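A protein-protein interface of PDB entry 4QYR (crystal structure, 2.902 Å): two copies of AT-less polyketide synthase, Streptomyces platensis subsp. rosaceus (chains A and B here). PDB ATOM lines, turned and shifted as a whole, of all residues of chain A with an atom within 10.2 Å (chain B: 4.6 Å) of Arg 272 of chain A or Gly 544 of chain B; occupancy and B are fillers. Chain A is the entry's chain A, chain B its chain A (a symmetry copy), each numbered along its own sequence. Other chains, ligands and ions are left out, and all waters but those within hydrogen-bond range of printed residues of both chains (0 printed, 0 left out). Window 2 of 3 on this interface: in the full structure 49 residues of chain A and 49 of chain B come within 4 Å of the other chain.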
ATOM      1  N   HIS A 269      13.389  27.627  -9.691  1.00  0.00           N
ATOM      2  CA  HIS A 269      12.180  28.347 -10.003  1.00  0.00           C
ATOM      3  C   HIS A 269      11.444  27.625 -11.098  1.00  0.00           C
ATOM      4  O   HIS A 269      12.044  26.939 -11.912  1.00  0.00           O
ATOM      5  CB  HIS A 269      12.464  29.785 -10.417  1.00  0.00           C
ATOM      6  CG  HIS A 269      11.223  30.586 -10.668  1.00  0.00           C
ATOM      7  ND1 HIS A 269      10.598  30.627 -11.896  1.00  0.00           N
ATOM      8  CD2 HIS A 269      10.490  31.378  -9.850  1.00  0.00           C
ATOM      9  CE1 HIS A 269       9.536  31.409 -11.822  1.00  0.00           C
ATOM     10  NE2 HIS A 269       9.444  31.873 -10.591  1.00  0.00           N
ATOM     11  N   GLY A 270      10.129  27.794 -11.098  1.00  0.00           N
ATOM     12  CA  GLY A 270       9.251  27.113 -12.026  1.00  0.00           C
ATOM     13  C   GLY A 270       9.404  27.457 -13.491  1.00  0.00           C
ATOM     14  O   GLY A 270       9.099  26.619 -14.326  1.00  0.00           O
ATOM     15  N   GLY A 271       9.872  28.661 -13.816  1.00  0.00           N
ATOM     16  CA  GLY A 271       9.937  29.096 -15.208  1.00  0.00           C
ATOM     17  C   GLY A 271       8.535  29.290 -15.762  1.00  0.00           C
ATOM     18  O   GLY A 271       7.662  29.731 -15.045  1.00  0.00           O
ATOM     19  N   ARG A 272       8.294  28.941 -17.021  1.00  0.00           N
ATOM     20  CA  ARG A 272       6.950  29.128 -17.579  1.00  0.00           C
ATOM     21  C   ARG A 272       6.054  27.923 -17.337  1.00  0.00           C
ATOM     22  O   ARG A 272       6.239  26.856 -17.927  1.00  0.00           O
ATOM     23  CB  ARG A 272       7.000  29.437 -19.068  1.00  0.00           C
ATOM     24  CG  ARG A 272       6.512  30.836 -19.380  1.00  0.00           C
ATOM     25  CD  ARG A 272       6.188  30.944 -20.837  1.00  0.00           C
ATOM     26  NE  ARG A 272       5.988  32.314 -21.274  1.00  0.00           N
ATOM     27  CZ  ARG A 272       6.942  33.072 -21.786  1.00  0.00           C
ATOM     28  NH1 ARG A 272       8.162  32.585 -21.936  1.00  0.00           N
ATOM     29  NH2 ARG A 272       6.663  34.311 -22.165  1.00  0.00           N
ATOM     30  N   ALA A 273       5.057  28.129 -16.482  1.00  0.00           N
ATOM     31  CA  ALA A 273       4.248  27.043 -15.959  1.00  0.00           C
ATOM     32  C   ALA A 273       2.793  27.067 -16.434  1.00  0.00           C
ATOM     33  O   ALA A 273       1.953  26.317 -15.925  1.00  0.00           O
ATOM     34  CB  ALA A 273       4.293  27.066 -14.433  1.00  0.00           C
ATOM     35  N   GLY A 274       2.483  27.917 -17.396  1.00  0.00           N
ATOM     36  CA  GLY A 274       1.115  27.979 -17.874  1.00  0.00           C
ATOM     37  C   GLY A 274       0.433  29.236 -17.393  1.00  0.00           C
ATOM     38  O   GLY A 274      -0.252  29.930 -18.159  1.00  0.00           O
ATOM     39  N   SER A 275       0.607  29.514 -16.108  1.00  0.00           N
ATOM     40  CA  SER A 275       0.321  30.834 -15.581  1.00  0.00           C
ATOM     41  C   SER A 275       1.292  31.149 -14.448  1.00  0.00           C
ATOM     42  O   SER A 275       1.985  30.265 -13.922  1.00  0.00           O
ATOM     43  CB  SER A 275      -1.124  30.949 -15.103  1.00  0.00           C
ATOM     44  OG  SER A 275      -1.432  29.948 -14.160  1.00  0.00           O
ATOM     45  N   LEU A 276       1.330  32.425 -14.096  1.00  0.00           N
ATOM     46  CA  LEU A 276       2.236  32.941 -13.097  1.00  0.00           C
ATOM     47  C   LEU A 276       2.194  32.108 -11.819  1.00  0.00           C
ATOM     48  O   LEU A 276       3.236  31.796 -11.235  1.00  0.00           O
ATOM     49  CB  LEU A 276       1.887  34.406 -12.811  1.00  0.00           C
ATOM     50  CG  LEU A 276       2.919  35.279 -12.103  1.00  0.00           C
ATOM     51  CD1 LEU A 276       4.275  35.041 -12.726  1.00  0.00           C
ATOM     52  CD2 LEU A 276       2.520  36.765 -12.158  1.00  0.00           C
ATOM     53  N   THR A 277       0.989  31.714 -11.412  1.00  0.00           N
ATOM     54  CA  THR A 277       0.788  31.107 -10.098  1.00  0.00           C
ATOM     55  C   THR A 277       0.327  29.649 -10.155  1.00  0.00           C
ATOM     56  O   THR A 277      -0.091  29.085  -9.139  1.00  0.00           O
ATOM     57  CB  THR A 277      -0.230  31.911  -9.297  1.00  0.00           C
ATOM     58  OG1 THR A 277      -1.488  31.868  -9.982  1.00  0.00           O
ATOM     59  CG2 THR A 277       0.222  33.364  -9.183  1.00  0.00           C
ATOM     60  N   ALA A 278       0.401  29.042 -11.337  1.00  0.00           N
ATOM     61  CA  ALA A 278       0.177  27.600 -11.490  1.00  0.00           C
ATOM     62  C   ALA A 278       1.379  26.767 -11.007  1.00  0.00           C
ATOM     63  O   ALA A 278       2.531  27.187 -11.148  1.00  0.00           O
ATOM     64  CB  ALA A 278      -0.129  27.276 -12.938  1.00  0.00           C
ATOM     65  N   PRO A 279       1.116  25.579 -10.438  1.00  0.00           N
ATOM     66  CA  PRO A 279       2.199  24.694  -9.998  1.00  0.00           C
ATOM     67  C   PRO A 279       2.844  23.977 -11.183  1.00  0.00           C
ATOM     68  O   PRO A 279       2.170  23.668 -12.164  1.00  0.00           O
ATOM     69  CB  PRO A 279       1.483  23.709  -9.074  1.00  0.00           C
ATOM     70  CG  PRO A 279       0.117  23.591  -9.662  1.00  0.00           C
ATOM     71  CD  PRO A 279      -0.209  24.961 -10.242  1.00  0.00           C
ATOM     72  N   ASN A 280       4.145  23.739 -11.098  1.00  0.00           N
ATOM     73  CA  ASN A 280       4.877  23.127 -12.199  1.00  0.00           C
ATOM     74  C   ASN A 280       5.522  21.849 -11.726  1.00  0.00           C
ATOM     75  O   ASN A 280       6.604  21.866 -11.150  1.00  0.00           O
ATOM     76  CB  ASN A 280       5.923  24.085 -12.760  1.00  0.00           C
ATOM     77  CG  ASN A 280       6.717  23.491 -13.920  1.00  0.00           C
ATOM     78  OD1 ASN A 280       6.741  22.279 -14.136  1.00  0.00           O
ATOM     79  ND2 ASN A 280       7.367  24.356 -14.681  1.00  0.00           N
ATOM     80  N   GLY A 281       4.847  20.738 -12.007  1.00  0.00           N
ATOM     81  CA  GLY A 281       5.285  19.432 -11.564  1.00  0.00           C
ATOM     82  C   GLY A 281       6.672  19.033 -12.014  1.00  0.00           C
ATOM     83  O   GLY A 281       7.401  18.415 -11.254  1.00  0.00           O
ATOM     84  N   LYS A 282       7.050  19.382 -13.237  1.00  0.00           N
ATOM     85  CA  LYS A 282       8.338  18.939 -13.729  1.00  0.00           C
ATOM     86  C   LYS A 282       9.445  19.717 -13.044  1.00  0.00           C
ATOM     87  O   LYS A 282      10.540  19.195 -12.852  1.00  0.00           O
ATOM     88  CB  LYS A 282       8.447  19.057 -15.248  1.00  0.00           C
ATOM     89  CG  LYS A 282       9.400  17.991 -15.772  1.00  0.00           C
ATOM     90  CD  LYS A 282       9.393  17.760 -17.285  1.00  0.00           C
ATOM     91  CE  LYS A 282      10.299  16.539 -17.596  1.00  0.00           C
ATOM     92  NZ  LYS A 282      10.671  16.336 -19.028  1.00  0.00           N
ATOM     93  N   ALA A 283       9.154  20.947 -12.633  1.00  0.00           N
ATOM     94  CA  ALA A 283      10.103  21.714 -11.826  1.00  0.00           C
ATOM     95  C   ALA A 283      10.184  21.189 -10.399  1.00  0.00           C
ATOM     96  O   ALA A 283      11.268  21.125  -9.820  1.00  0.00           O
ATOM     97  CB  ALA A 283       9.727  23.186 -11.810  1.00  0.00           C
ATOM     98  N   GLY A 426       4.654  32.367  -6.571  1.00  0.00           N
ATOM     99  CA  GLY A 426       5.304  32.877  -7.758  1.00  0.00           C
ATOM    100  C   GLY A 426       6.179  31.905  -8.516  1.00  0.00           C
ATOM    101  O   GLY A 426       6.708  32.253  -9.572  1.00  0.00           O
ATOM    102  N   GLY A 427       6.358  30.701  -7.987  1.00  0.00           N
ATOM    103  CA  GLY A 427       7.123  29.692  -8.687  1.00  0.00           C
ATOM    104  C   GLY A 427       8.481  29.412  -8.089  1.00  0.00           C
ATOM    105  O   GLY A 427       9.268  28.676  -8.697  1.00  0.00           O
ATOM    106  N   ALA A 428       8.768  29.996  -6.918  1.00  0.00           N
ATOM    107  CA  ALA A 428      10.042  29.740  -6.242  1.00  0.00           C
ATOM    108  C   ALA A 428       9.902  28.590  -5.265  1.00  0.00           C
ATOM    109  O   ALA A 428       9.100  28.657  -4.337  1.00  0.00           O
ATOM    110  CB  ALA A 428      10.538  30.984  -5.525  1.00  0.00           C
ATOM    111  N   ASN A 429      10.688  27.540  -5.475  1.00  0.00           N
ATOM    112  CA  ASN A 429      10.533  26.310  -4.718  1.00  0.00           C
ATOM    113  C   ASN A 429      11.781  25.917  -3.982  1.00  0.00           C
ATOM    114  O   ASN A 429      12.890  26.044  -4.508  1.00  0.00           O
ATOM    115  CB  ASN A 429      10.143  25.154  -5.628  1.00  0.00           C
ATOM    116  CG  ASN A 429       9.157  25.551  -6.679  1.00  0.00           C
ATOM    117  OD1 ASN A 429       8.147  26.205  -6.397  1.00  0.00           O
ATOM    118  ND2 ASN A 429       9.430  25.148  -7.913  1.00  0.00           N
ATOM    119  N   TYR B 158       9.585  33.838 -14.850  1.00  0.00           N
ATOM    120  CA  TYR B 158       8.424  33.378 -15.627  1.00  0.00           C
ATOM    121  C   TYR B 158       8.523  33.841 -17.085  1.00  0.00           C
ATOM    122  O   TYR B 158       8.333  33.063 -18.015  1.00  0.00           O
ATOM    123  CB  TYR B 158       7.133  33.881 -15.006  1.00  0.00           C
ATOM    124  CG  TYR B 158       5.872  33.492 -15.745  1.00  0.00           C
ATOM    125  CD1 TYR B 158       5.270  32.270 -15.529  1.00  0.00           C
ATOM    126  CD2 TYR B 158       5.272  34.358 -16.659  1.00  0.00           C
ATOM    127  CE1 TYR B 158       4.111  31.910 -16.196  1.00  0.00           C
ATOM    128  CE2 TYR B 158       4.113  34.004 -17.347  1.00  0.00           C
ATOM    129  CZ  TYR B 158       3.538  32.777 -17.103  1.00  0.00           C
ATOM    130  OH  TYR B 158       2.387  32.390 -17.756  1.00  0.00           O
ATOM    131  N   VAL B 159       8.838  35.112 -17.291  1.00  0.00           N
ATOM    132  CA  VAL B 159       8.947  35.637 -18.654  1.00  0.00           C
ATOM    133  C   VAL B 159      10.062  34.951 -19.457  1.00  0.00           C
ATOM    134  O   VAL B 159       9.890  34.663 -20.630  1.00  0.00           O
ATOM    135  CB  VAL B 159       9.163  37.161 -18.638  1.00  0.00           C
ATOM    136  CG1 VAL B 159       9.693  37.640 -19.951  1.00  0.00           C
ATOM    137  CG2 VAL B 159       7.846  37.862 -18.310  1.00  0.00           C
ATOM    138  N   ASP B 161      11.420  31.938 -18.776  1.00  0.00           N
ATOM    139  CA  ASP B 161      11.400  30.488 -18.591  1.00  0.00           C
ATOM    140  C   ASP B 161      12.751  29.941 -18.130  1.00  0.00           C
ATOM    141  O   ASP B 161      13.310  29.039 -18.736  1.00  0.00           O
ATOM    142  CB  ASP B 161      10.955  29.778 -19.876  1.00  0.00           C
ATOM    143  CG  ASP B 161      10.803  28.259 -19.700  1.00  0.00           C
ATOM    144  OD1 ASP B 161      10.326  27.803 -18.630  1.00  0.00           O
ATOM    145  OD2 ASP B 161      11.182  27.517 -20.640  1.00  0.00           O
ATOM    146  N   GLY B 544       5.466  28.283 -24.087  1.00  0.00           N
ATOM    147  CA  GLY B 544       6.739  28.329 -23.382  1.00  0.00           C
ATOM    148  C   GLY B 544       7.904  28.704 -24.285  1.00  0.00           C
ATOM    149  O   GLY B 544       7.701  29.055 -25.451  1.00  0.00           O
ATOM    150  N   VAL B 545       9.123  28.634 -23.749  1.00  0.00           N
ATOM    151  CA  VAL B 545      10.336  28.916 -24.529  1.00  0.00           C
ATOM    152  C   VAL B 545      11.042  27.627 -24.972  1.00  0.00           C
ATOM    153  O   VAL B 545      11.551  26.868 -24.140  1.00  0.00           O
ATOM    154  CB  VAL B 545      11.351  29.785 -23.728  1.00  0.00           C
ATOM    155  CG1 VAL B 545      12.710  29.819 -24.421  1.00  0.00           C
ATOM    156  CG2 VAL B 545      10.816  31.205 -23.504  1.00  0.00           C
ATOM    157  N   ARG B 546      11.076  27.389 -26.282  1.00  0.00           N
ATOM    158  CA  ARG B 546      11.747  26.207 -26.828  1.00  0.00           C
ATOM    159  C   ARG B 546      13.242  26.438 -27.034  1.00  0.00           C
ATOM    160  O   ARG B 546      13.660  27.014 -28.036  1.00  0.00           O
ATOM    161  CB  ARG B 546      11.103  25.772 -28.150  1.00  0.00           C
ATOM    162  CG  ARG B 546      11.577  24.400 -28.642  1.00  0.00           C
ATOM    163  CD  ARG B 546      10.605  23.740 -29.624  1.00  0.00           C
ATOM    164  NE  ARG B 546       9.687  24.692 -30.245  1.00  0.00           N
ATOM    165  CZ  ARG B 546       8.376  24.496 -30.373  1.00  0.00           C
ATOM    166  NH1 ARG B 546       7.821  23.374 -29.932  1.00  0.00           N
ATOM    167  NH2 ARG B 546       7.620  25.419 -30.953  1.00  0.00           N
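Among the printed residues, pairs that only touch across the chains: His 269 of chain A with Tyr 158 of chain B (3.9 Å), Gly 271 of chain A with Tyr 158 of chain B (3.5 Å), Gly 271 of chain A with Asp 161 of chain B (3.7 Å), Arg 272 of chain A with Tyr 158 of chain B (3.2 Å), Arg 272 of chain A with Gly 544 of chain B (3.7 Å), Arg 272 of chain A with Val 545 of chain B (3.4 Å), Ala 273 of chain A with Tyr 158 of chain B (3.9 Å), Gly 274 of chain A with Tyr 158 of chain B (3.6 Å), Ser 275 of chain A with Tyr 158 of chain B (3.4 Å) and Leu 276 of chain A with Tyr 158 of chain B (3.5 Å).
Printed residues of chain A that touch a printed residue of chain B: His 269, Gly 271, Arg 272, Ala 273, Gly 274, Ser 275 and Leu 276.
Of the 6 printed residues of chain B, 5 touch a printed residue of chain A.
Printed residues of chain B that touch a printed residue of chain A: Tyr 158, Val 159, Asp 161, Gly 544 and Val 545.
Hydrophobic or aromatic side chains of chain B that line the printed part of chain A: Tyr 158 and Val 545.
Among the printed residues, 12 pairs touch across the chains.
NE2 of His 269 of chain A is in hydrogen-bond range of O of Gly 426 of chain A.
A ring nitrogen (ND1) of His 269 of chain A lies within hydrogen-bond range of the backbone NH (N) of Gly 271 of chain A, 2.8 Å away.
The side-chain hydroxyl (OG) of Ser 275 of chain A sits close to the backbone NH (N) of Ala 278 of chain A (3.5 Å).
Arg 272 of chain A touches five residues of chain B.
Of chain A, only Arg 272 (3.7 Å) comes within 4 Å of Gly 544 of chain B.
Tyr 158 of chain B touches just these residues of chain A: His 269, Gly 271, Arg 272, Ala 273, Gly 274, Ser 275 and Leu 276.
Val 159 of chain B touches just one residue of chain A: Arg 272.
Val 545 of chain B touches just one residue of chain A: Arg 272.
Of the printed residues of chain B, Gly 274 of chain A touches Tyr 158 (3.6 Å).
Printed residues of chain B within 4 Å of Gly 271 of chain A: Tyr 158 and Asp 161.
Printed residues of chain B within 4 Å of His 269 of chain A: Tyr 158.
Printed residues of chain B within 4 Å of Ala 273 of chain A: Tyr 158.
Printed residues of chain B within 4 Å of Leu 276 of chain A: Tyr 158 (3.5 Å).
The nearest printed residue of chain B that does not touch Arg 272 of chain A is Arg 546 of chain B (7.4 Å).
No position is printed for both chains.
Of the 12 pairs that touch across the chains among the printed residues, none has its exchanged pair printed and touching as well.
OD1 of Asp 161 of chain B sits at hydrogen-bond distance from N of Arg 272 of chain A.
NH1 of Arg 272 of chain A lies within hydrogen-bond range of O of Val 159 of chain B, at 3.0 Å.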
